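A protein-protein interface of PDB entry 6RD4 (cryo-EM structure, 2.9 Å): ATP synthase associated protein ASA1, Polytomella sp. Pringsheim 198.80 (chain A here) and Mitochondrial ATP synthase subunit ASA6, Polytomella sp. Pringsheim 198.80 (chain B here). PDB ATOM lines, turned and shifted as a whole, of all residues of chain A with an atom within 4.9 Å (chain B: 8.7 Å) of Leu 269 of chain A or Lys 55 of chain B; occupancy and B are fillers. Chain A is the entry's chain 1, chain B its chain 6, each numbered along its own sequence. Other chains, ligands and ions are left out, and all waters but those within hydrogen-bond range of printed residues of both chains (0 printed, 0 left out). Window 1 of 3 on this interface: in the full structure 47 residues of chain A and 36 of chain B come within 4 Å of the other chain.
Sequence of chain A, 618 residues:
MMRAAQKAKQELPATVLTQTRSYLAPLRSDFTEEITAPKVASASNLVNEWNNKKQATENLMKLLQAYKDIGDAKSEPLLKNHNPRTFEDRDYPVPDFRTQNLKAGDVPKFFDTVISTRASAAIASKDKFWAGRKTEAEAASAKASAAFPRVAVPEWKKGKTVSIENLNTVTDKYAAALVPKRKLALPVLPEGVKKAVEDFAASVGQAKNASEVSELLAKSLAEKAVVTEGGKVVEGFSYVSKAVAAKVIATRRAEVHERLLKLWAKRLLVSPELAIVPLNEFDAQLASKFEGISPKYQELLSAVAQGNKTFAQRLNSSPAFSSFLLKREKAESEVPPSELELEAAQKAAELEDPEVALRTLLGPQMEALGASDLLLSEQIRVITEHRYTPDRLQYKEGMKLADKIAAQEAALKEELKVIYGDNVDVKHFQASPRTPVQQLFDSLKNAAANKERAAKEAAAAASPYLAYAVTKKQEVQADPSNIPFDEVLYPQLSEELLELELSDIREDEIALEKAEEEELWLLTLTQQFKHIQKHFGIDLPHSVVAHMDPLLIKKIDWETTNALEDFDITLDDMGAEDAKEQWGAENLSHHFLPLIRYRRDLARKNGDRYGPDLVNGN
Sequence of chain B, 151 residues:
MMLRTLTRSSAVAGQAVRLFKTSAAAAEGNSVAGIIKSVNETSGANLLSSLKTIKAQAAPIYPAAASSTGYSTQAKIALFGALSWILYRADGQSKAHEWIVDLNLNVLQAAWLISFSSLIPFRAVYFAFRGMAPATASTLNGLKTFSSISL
The backbone carbonyl oxygen (O) of Leu 269 of chain A sits at hydrogen-bond distance from the side-chain amino group (NZ) of Lys 55 of chain B (3.3 Å).
Among the printed residues, merely in contact across the chains: Pro 354 of chain A with Leu 51 of chain B, Leu 269 of chain A with Leu 51 of chain B, Leu 269 of chain A with Ile 54 of chain B, Val 270 of chain A with Val 32 of chain B, Lys 266 of chain A with Ile 36 of chain B, Val 270 of chain A with Ile 35 of chain B and Ala 265 of chain A with Val 39 of chain B.
Printed residues of chain B within 4 Å of Lys 266 of chain A: Ile 36 (3.98 Å). Printed residues of chain B within 4 Å of Leu 269 of chain A: Leu 51, Ile 54 and Lys 55. Printed residues of chain B within 4 Å of Pro 354 of chain A: Leu 51. Of the printed residues of chain A, Val 32 of chain B touches Val 270. Of the printed residues of chain A, Ile 35 of chain B touches Val 270 (3.98 Å). Of the printed residues of chain A, Ile 54 of chain B touches Leu 269. Lys 55 of chain B touches just one residue of chain A: Leu 269 (3.3 Å). The nearest printed residue of chain B that does not touch Leu 269 of chain A is Ile 35 of chain B (4.01 Å). The nearest printed residue of chain B that does not touch Ala 265 of chain A is Leu 51 of chain B (4.04 Å).
Of the 20 printed residues of chain B, 7 touch a printed residue of chain A. Printed residues of chain B that touch a printed residue of chain A: Val 32, Ile 35, Ile 36, Val 39, Leu 51, Ile 54 and Lys 55. Hydrophobic or aromatic side chains of chain B within 4 Å of the printed part of chain A: Val 32, Ile 35, Ile 36, Val 39, Leu 51 and Ile 54. Along chain B the printed residues that touch a printed residue of chain A span positions 32 to 55. Among the printed residues, no Asp or Glu carboxylate lies within 4 Å of a Lys or Arg side-chain nitrogen of the other chain.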
ATOM      1  N   ALA A 265      23.619  -4.603 -22.613  1.00  0.00           N
ATOM      2  CA  ALA A 265      22.891  -4.655 -21.357  1.00  0.00           C
ATOM      3  C   ALA A 265      22.855  -6.064 -20.812  1.00  0.00           C
ATOM      4  O   ALA A 265      23.023  -6.263 -19.615  1.00  0.00           O
ATOM      5  CB  ALA A 265      21.478  -4.133 -21.535  1.00  0.00           C
ATOM      6  N   LYS A 266      22.666  -7.055 -21.675  1.00  0.00           N
ATOM      7  CA  LYS A 266      22.647  -8.434 -21.217  1.00  0.00           C
ATOM      8  C   LYS A 266      24.024  -8.911 -20.812  1.00  0.00           C
ATOM      9  O   LYS A 266      24.153  -9.719 -19.898  1.00  0.00           O
ATOM     10  CB  LYS A 266      22.104  -9.337 -22.303  1.00  0.00           C
ATOM     11  CG  LYS A 266      20.878  -8.839 -22.938  1.00  0.00           C
ATOM     12  CD  LYS A 266      20.676  -9.537 -24.217  1.00  0.00           C
ATOM     13  CE  LYS A 266      19.563  -8.934 -24.985  1.00  0.00           C
ATOM     14  NZ  LYS A 266      19.488  -9.528 -26.322  1.00  0.00           N
ATOM     15  N   ARG A 267      25.054  -8.439 -21.472  1.00  0.00           N
ATOM     16  CA  ARG A 267      26.385  -8.938 -21.209  1.00  0.00           C
ATOM     17  C   ARG A 267      26.963  -8.339 -19.955  1.00  0.00           C
ATOM     18  O   ARG A 267      27.907  -8.890 -19.404  1.00  0.00           O
ATOM     19  CB  ARG A 267      27.307  -8.635 -22.381  1.00  0.00           C
ATOM     20  CG  ARG A 267      27.387  -9.692 -23.427  1.00  0.00           C
ATOM     21  CD  ARG A 267      26.168  -9.703 -24.238  1.00  0.00           C
ATOM     22  NE  ARG A 267      26.280 -10.506 -25.420  1.00  0.00           N
ATOM     23  CZ  ARG A 267      25.255 -10.819 -26.179  1.00  0.00           C
ATOM     24  NH1 ARG A 267      24.058 -10.398 -25.855  1.00  0.00           N
ATOM     25  NH2 ARG A 267      25.422 -11.571 -27.239  1.00  0.00           N
ATOM     26  N   LEU A 268      26.430  -7.214 -19.508  1.00  0.00           N
ATOM     27  CA  LEU A 268      26.868  -6.568 -18.293  1.00  0.00           C
ATOM     28  C   LEU A 268      25.895  -6.752 -17.149  1.00  0.00           C
ATOM     29  O   LEU A 268      26.181  -6.303 -16.042  1.00  0.00           O
ATOM     30  CB  LEU A 268      27.091  -5.074 -18.538  1.00  0.00           C
ATOM     31  CG  LEU A 268      28.220  -4.724 -19.496  1.00  0.00           C
ATOM     32  CD1 LEU A 268      28.060  -3.332 -19.943  1.00  0.00           C
ATOM     33  CD2 LEU A 268      29.534  -4.854 -18.828  1.00  0.00           C
ATOM     34  N   LEU A 269      24.749  -7.365 -17.388  1.00  0.00           N
ATOM     35  CA  LEU A 269      23.922  -7.825 -16.287  1.00  0.00           C
ATOM     36  C   LEU A 269      24.379  -9.193 -15.825  1.00  0.00           C
ATOM     37  O   LEU A 269      24.425  -9.465 -14.624  1.00  0.00           O
ATOM     38  CB  LEU A 269      22.463  -7.874 -16.711  1.00  0.00           C
ATOM     39  CG  LEU A 269      21.697  -6.565 -16.689  1.00  0.00           C
ATOM     40  CD1 LEU A 269      20.327  -6.780 -17.229  1.00  0.00           C
ATOM     41  CD2 LEU A 269      21.634  -6.076 -15.322  1.00  0.00           C
ATOM     42  N   VAL A 270      24.722 -10.058 -16.771  1.00  0.00           N
ATOM     43  CA  VAL A 270      25.278 -11.358 -16.431  1.00  0.00           C
ATOM     44  C   VAL A 270      26.712 -11.210 -15.964  1.00  0.00           C
ATOM     45  O   VAL A 270      27.085 -11.685 -14.889  1.00  0.00           O
ATOM     46  CB  VAL A 270      25.180 -12.295 -17.639  1.00  0.00           C
ATOM     47  CG1 VAL A 270      25.981 -13.505 -17.402  1.00  0.00           C
ATOM     48  CG2 VAL A 270      23.762 -12.659 -17.892  1.00  0.00           C
ATOM     49  N   SER A 271      27.534 -10.530 -16.749  1.00  0.00           N
ATOM     50  CA  SER A 271      28.978 -10.530 -16.579  1.00  0.00           C
ATOM     51  C   SER A 271      29.502  -9.106 -16.502  1.00  0.00           C
ATOM     52  O   SER A 271      30.125  -8.626 -17.453  1.00  0.00           O
ATOM     53  CB  SER A 271      29.634 -11.262 -17.742  1.00  0.00           C
ATOM     54  OG  SER A 271      31.017 -11.056 -17.723  1.00  0.00           O
ATOM     55  N   PRO A 272      29.324  -8.418 -15.372  1.00  0.00           N
ATOM     56  CA  PRO A 272      29.646  -6.990 -15.327  1.00  0.00           C
ATOM     57  C   PRO A 272      31.118  -6.682 -15.287  1.00  0.00           C
ATOM     58  O   PRO A 272      31.482  -5.512 -15.383  1.00  0.00           O
ATOM     59  CB  PRO A 272      28.967  -6.529 -14.045  1.00  0.00           C
ATOM     60  CG  PRO A 272      28.964  -7.685 -13.218  1.00  0.00           C
ATOM     61  CD  PRO A 272      28.746  -8.862 -14.102  1.00  0.00           C
ATOM     62  N   GLU A 352      28.462  -3.077  -9.925  1.00  0.00           N
ATOM     63  CA  GLU A 352      27.186  -3.710  -9.626  1.00  0.00           C
ATOM     64  C   GLU A 352      26.012  -2.833 -10.010  1.00  0.00           C
ATOM     65  O   GLU A 352      24.874  -3.308  -9.992  1.00  0.00           O
ATOM     66  CB  GLU A 352      27.069  -4.086  -8.147  1.00  0.00           C
ATOM     67  CG  GLU A 352      28.051  -5.140  -7.673  1.00  0.00           C
ATOM     68  CD  GLU A 352      28.063  -6.400  -8.532  1.00  0.00           C
ATOM     69  OE1 GLU A 352      29.057  -6.619  -9.253  1.00  0.00           O
ATOM     70  OE2 GLU A 352      27.092  -7.181  -8.477  1.00  0.00           O
ATOM     71  N   PRO A 354      24.511  -1.642 -13.180  1.00  0.00           N
ATOM     72  CA  PRO A 354      24.698  -1.950 -14.597  1.00  0.00           C
ATOM     73  C   PRO A 354      24.641  -0.736 -15.499  1.00  0.00           C
ATOM     74  O   PRO A 354      25.030  -0.845 -16.663  1.00  0.00           O
ATOM     75  CB  PRO A 354      23.561  -2.929 -14.891  1.00  0.00           C
ATOM     76  CG  PRO A 354      22.573  -2.667 -13.867  1.00  0.00           C
ATOM     77  CD  PRO A 354      23.249  -2.172 -12.660  1.00  0.00           C
ATOM     78  N   SER B  31      17.573 -17.787 -15.551  1.00  0.00           N
ATOM     79  CA  SER B  31      17.493 -16.360 -15.339  1.00  0.00           C
ATOM     80  C   SER B  31      18.158 -15.565 -16.429  1.00  0.00           C
ATOM     81  O   SER B  31      17.945 -14.362 -16.507  1.00  0.00           O
ATOM     82  CB  SER B  31      18.138 -15.994 -14.023  1.00  0.00           C
ATOM     83  OG  SER B  31      19.525 -16.177 -14.096  1.00  0.00           O
ATOM     84  N   VAL B  32      18.980 -16.189 -17.252  1.00  0.00           N
ATOM     85  CA  VAL B  32      19.555 -15.465 -18.370  1.00  0.00           C
ATOM     86  C   VAL B  32      18.530 -15.303 -19.474  1.00  0.00           C
ATOM     87  O   VAL B  32      18.420 -14.234 -20.071  1.00  0.00           O
ATOM     88  CB  VAL B  32      20.828 -16.173 -18.837  1.00  0.00           C
ATOM     89  CG1 VAL B  32      21.389 -15.496 -20.007  1.00  0.00           C
ATOM     90  CG2 VAL B  32      21.818 -16.107 -17.752  1.00  0.00           C
ATOM     91  N   GLY B  34      15.511 -15.035 -18.741  1.00  0.00           N
ATOM     92  CA  GLY B  34      14.693 -13.991 -18.171  1.00  0.00           C
ATOM     93  C   GLY B  34      15.305 -12.622 -18.322  1.00  0.00           C
ATOM     94  O   GLY B  34      14.588 -11.632 -18.392  1.00  0.00           O
ATOM     95  N   ILE B  35      16.633 -12.540 -18.346  1.00  0.00           N
ATOM     96  CA  ILE B  35      17.305 -11.271 -18.599  1.00  0.00           C
ATOM     97  C   ILE B  35      17.136 -10.879 -20.051  1.00  0.00           C
ATOM     98  O   ILE B  35      16.824  -9.731 -20.362  1.00  0.00           O
ATOM     99  CB  ILE B  35      18.790 -11.374 -18.212  1.00  0.00           C
ATOM    100  CG1 ILE B  35      18.967 -11.174 -16.724  1.00  0.00           C
ATOM    101  CG2 ILE B  35      19.630 -10.358 -18.911  1.00  0.00           C
ATOM    102  CD1 ILE B  35      20.370 -11.370 -16.259  1.00  0.00           C
ATOM    103  N   ILE B  36      17.328 -11.834 -20.956  1.00  0.00           N
ATOM    104  CA  ILE B  36      17.227 -11.587 -22.386  1.00  0.00           C
ATOM    105  C   ILE B  36      15.818 -11.171 -22.759  1.00  0.00           C
ATOM    106  O   ILE B  36      15.629 -10.252 -23.554  1.00  0.00           O
ATOM    107  CB  ILE B  36      17.677 -12.839 -23.153  1.00  0.00           C
ATOM    108  CG1 ILE B  36      19.177 -13.021 -23.027  1.00  0.00           C
ATOM    109  CG2 ILE B  36      17.295 -12.778 -24.589  1.00  0.00           C
ATOM    110  CD1 ILE B  36      19.666 -14.239 -23.661  1.00  0.00           C
ATOM    111  N   SER B  38      13.509  -9.763 -20.639  1.00  0.00           N
ATOM    112  CA  SER B  38      13.203  -8.489 -20.006  1.00  0.00           C
ATOM    113  C   SER B  38      13.956  -7.319 -20.603  1.00  0.00           C
ATOM    114  O   SER B  38      13.532  -6.181 -20.424  1.00  0.00           O
ATOM    115  CB  SER B  38      13.522  -8.546 -18.524  1.00  0.00           C
ATOM    116  OG  SER B  38      12.609  -9.378 -17.846  1.00  0.00           O
ATOM    117  N   VAL B  39      15.079  -7.557 -21.259  1.00  0.00           N
ATOM    118  CA  VAL B  39      15.793  -6.478 -21.924  1.00  0.00           C
ATOM    119  C   VAL B  39      15.279  -6.297 -23.347  1.00  0.00           C
ATOM    120  O   VAL B  39      15.221  -5.175 -23.845  1.00  0.00           O
ATOM    121  CB  VAL B  39      17.306  -6.756 -21.855  1.00  0.00           C
ATOM    122  CG1 VAL B  39      18.093  -5.871 -22.728  1.00  0.00           C
ATOM    123  CG2 VAL B  39      17.794  -6.546 -20.467  1.00  0.00           C
ATOM    124  N   LEU B  47      15.384   1.805 -20.915  1.00  0.00           N
ATOM    125  CA  LEU B  47      16.337   0.711 -20.804  1.00  0.00           C
ATOM    126  C   LEU B  47      17.252   0.928 -19.620  1.00  0.00           C
ATOM    127  O   LEU B  47      17.395   0.053 -18.769  1.00  0.00           O
ATOM    128  CB  LEU B  47      17.160   0.576 -22.076  1.00  0.00           C
ATOM    129  CG  LEU B  47      18.367  -0.347 -21.925  1.00  0.00           C
ATOM    130  CD1 LEU B  47      17.911  -1.762 -21.829  1.00  0.00           C
ATOM    131  CD2 LEU B  47      19.308  -0.200 -23.064  1.00  0.00           C
ATOM    132  N   SER B  49      16.938   2.735 -17.031  1.00  0.00           N
ATOM    133  CA  SER B  49      16.284   2.722 -15.734  1.00  0.00           C
ATOM    134  C   SER B  49      15.888   1.323 -15.316  1.00  0.00           C
ATOM    135  O   SER B  49      15.868   1.028 -14.121  1.00  0.00           O
ATOM    136  CB  SER B  49      15.046   3.609 -15.754  1.00  0.00           C
ATOM    137  OG  SER B  49      13.945   2.914 -16.307  1.00  0.00           O
ATOM    138  N   SER B  50      15.592   0.454 -16.271  1.00  0.00           N
ATOM    139  CA  SER B  50      15.130  -0.882 -15.947  1.00  0.00           C
ATOM    140  C   SER B  50      16.254  -1.814 -15.556  1.00  0.00           C
ATOM    141  O   SER B  50      15.977  -2.943 -15.159  1.00  0.00           O
ATOM    142  CB  SER B  50      14.398  -1.489 -17.135  1.00  0.00           C
ATOM    143  OG  SER B  50      13.257  -0.734 -17.460  1.00  0.00           O
ATOM    144  N   LEU B  51      17.503  -1.393 -15.663  1.00  0.00           N
ATOM    145  CA  LEU B  51      18.583  -2.349 -15.547  1.00  0.00           C
ATOM    146  C   LEU B  51      18.849  -2.778 -14.120  1.00  0.00           C
ATOM    147  O   LEU B  51      19.512  -3.789 -13.925  1.00  0.00           O
ATOM    148  CB  LEU B  51      19.854  -1.786 -16.169  1.00  0.00           C
ATOM    149  CG  LEU B  51      19.919  -1.772 -17.691  1.00  0.00           C
ATOM    150  CD1 LEU B  51      21.325  -1.581 -18.131  1.00  0.00           C
ATOM    151  CD2 LEU B  51      19.335  -3.015 -18.293  1.00  0.00           C
ATOM    152  N   LYS B  52      18.340  -2.065 -13.124  1.00  0.00           N
ATOM    153  CA  LYS B  52      18.484  -2.520 -11.749  1.00  0.00           C
ATOM    154  C   LYS B  52      17.340  -3.396 -11.288  1.00  0.00           C
ATOM    155  O   LYS B  52      17.466  -4.050 -10.254  1.00  0.00           O
ATOM    156  CB  LYS B  52      18.617  -1.343 -10.795  1.00  0.00           C
ATOM    157  CG  LYS B  52      19.742  -0.425 -11.151  1.00  0.00           C
ATOM    158  CD  LYS B  52      20.274   0.317  -9.948  1.00  0.00           C
ATOM    159  CE  LYS B  52      21.177  -0.563  -9.122  1.00  0.00           C
ATOM    160  NZ  LYS B  52      21.984   0.249  -8.176  1.00  0.00           N
ATOM    161  N   THR B  53      16.225  -3.418 -12.001  1.00  0.00           N
ATOM    162  CA  THR B  53      15.151  -4.332 -11.669  1.00  0.00           C
ATOM    163  C   THR B  53      15.173  -5.579 -12.525  1.00  0.00           C
ATOM    164  O   THR B  53      14.449  -6.527 -12.224  1.00  0.00           O
ATOM    165  CB  THR B  53      13.791  -3.652 -11.821  1.00  0.00           C
ATOM    166  OG1 THR B  53      13.368  -3.725 -13.182  1.00  0.00           O
ATOM    167  CG2 THR B  53      13.897  -2.202 -11.426  1.00  0.00           C
ATOM    168  N   ILE B  54      15.951  -5.580 -13.601  1.00  0.00           N
ATOM    169  CA  ILE B  54      16.258  -6.809 -14.309  1.00  0.00           C
ATOM    170  C   ILE B  54      17.465  -7.472 -13.671  1.00  0.00           C
ATOM    171  O   ILE B  54      17.600  -8.695 -13.711  1.00  0.00           O
ATOM    172  CB  ILE B  54      16.464  -6.508 -15.802  1.00  0.00           C
ATOM    173  CG1 ILE B  54      15.242  -5.819 -16.367  1.00  0.00           C
ATOM    174  CG2 ILE B  54      16.627  -7.748 -16.600  1.00  0.00           C
ATOM    175  CD1 ILE B  54      15.450  -5.290 -17.733  1.00  0.00           C
ATOM    176  N   LYS B  55      18.339  -6.685 -13.051  1.00  0.00           N
ATOM    177  CA  LYS B  55      19.448  -7.243 -12.295  1.00  0.00           C
ATOM    178  C   LYS B  55      18.950  -8.005 -11.086  1.00  0.00           C
ATOM    179  O   LYS B  55      19.437  -9.097 -10.790  1.00  0.00           O
ATOM    180  CB  LYS B  55      20.380  -6.127 -11.853  1.00  0.00           C
ATOM    181  CG  LYS B  55      21.542  -6.539 -11.017  1.00  0.00           C
ATOM    182  CD  LYS B  55      22.666  -7.017 -11.871  1.00  0.00           C
ATOM    183  CE  LYS B  55      23.937  -7.109 -11.082  1.00  0.00           C
ATOM    184  NZ  LYS B  55      25.024  -7.707 -11.893  1.00  0.00           N
ATOM    185  N   ALA B  56      17.973  -7.451 -10.384  1.00  0.00           N
ATOM    186  CA  ALA B  56      17.467  -8.044  -9.161  1.00  0.00           C
ATOM    187  C   ALA B  56      16.398  -9.088  -9.405  1.00  0.00           C
ATOM    188  O   ALA B  56      16.089  -9.848  -8.495  1.00  0.00           O
ATOM    189  CB  ALA B  56      16.916  -6.956  -8.255  1.00  0.00           C
ATOM    190  N   GLN B  57      15.807  -9.130 -10.588  1.00  0.00           N
ATOM    191  CA  GLN B  57      14.899 -10.216 -10.910  1.00  0.00           C
ATOM    192  C   GLN B  57      15.636 -11.489 -11.261  1.00  0.00           C
ATOM    193  O   GLN B  57      15.022 -12.558 -11.292  1.00  0.00           O
ATOM    194  CB  GLN B  57      14.008  -9.834 -12.079  1.00  0.00           C
ATOM    195  CG  GLN B  57      12.664  -9.315 -11.693  1.00  0.00           C
ATOM    196  CD  GLN B  57      11.909  -8.755 -12.875  1.00  0.00           C
ATOM    197  OE1 GLN B  57      12.480  -8.532 -13.938  1.00  0.00           O
ATOM    198  NE2 GLN B  57      10.618  -8.516 -12.694  1.00  0.00           N
ATOM    199  N   ALA B  58      16.925 -11.393 -11.553  1.00  0.00           N
ATOM    200  CA  ALA B  58      17.740 -12.534 -11.925  1.00  0.00           C
ATOM    201  C   ALA B  58      18.862 -12.782 -10.941  1.00  0.00           C
ATOM    202  O   ALA B  58      19.758 -13.571 -11.233  1.00  0.00           O
ATOM    203  CB  ALA B  58      18.325 -12.334 -13.311  1.00  0.00           C
ATOM    204  N   ALA B  59      18.855 -12.101  -9.810  1.00  0.00           N
ATOM    205  CA  ALA B  59      19.747 -12.439  -8.733  1.00  0.00           C
ATOM    206  C   ALA B  59      19.311 -13.767  -8.134  1.00  0.00           C
ATOM    207  O   ALA B  59      18.131 -14.101  -8.171  1.00  0.00           O
ATOM    208  CB  ALA B  59      19.724 -11.350  -7.676  1.00  0.00           C
ATOM    209  N   PRO B  60      20.239 -14.560  -7.609  1.00  0.00           N
ATOM    210  CA  PRO B  60      19.844 -15.820  -6.988  1.00  0.00           C
ATOM    211  C   PRO B  60      19.198 -15.582  -5.640  1.00  0.00           C
ATOM    212  O   PRO B  60      19.414 -14.563  -4.988  1.00  0.00           O
ATOM    213  CB  PRO B  60      21.163 -16.564  -6.849  1.00  0.00           C
ATOM    214  CG  PRO B  60      22.140 -15.527  -6.768  1.00  0.00           C
ATOM    215  CD  PRO B  60      21.701 -14.441  -7.653  1.00  0.00           C
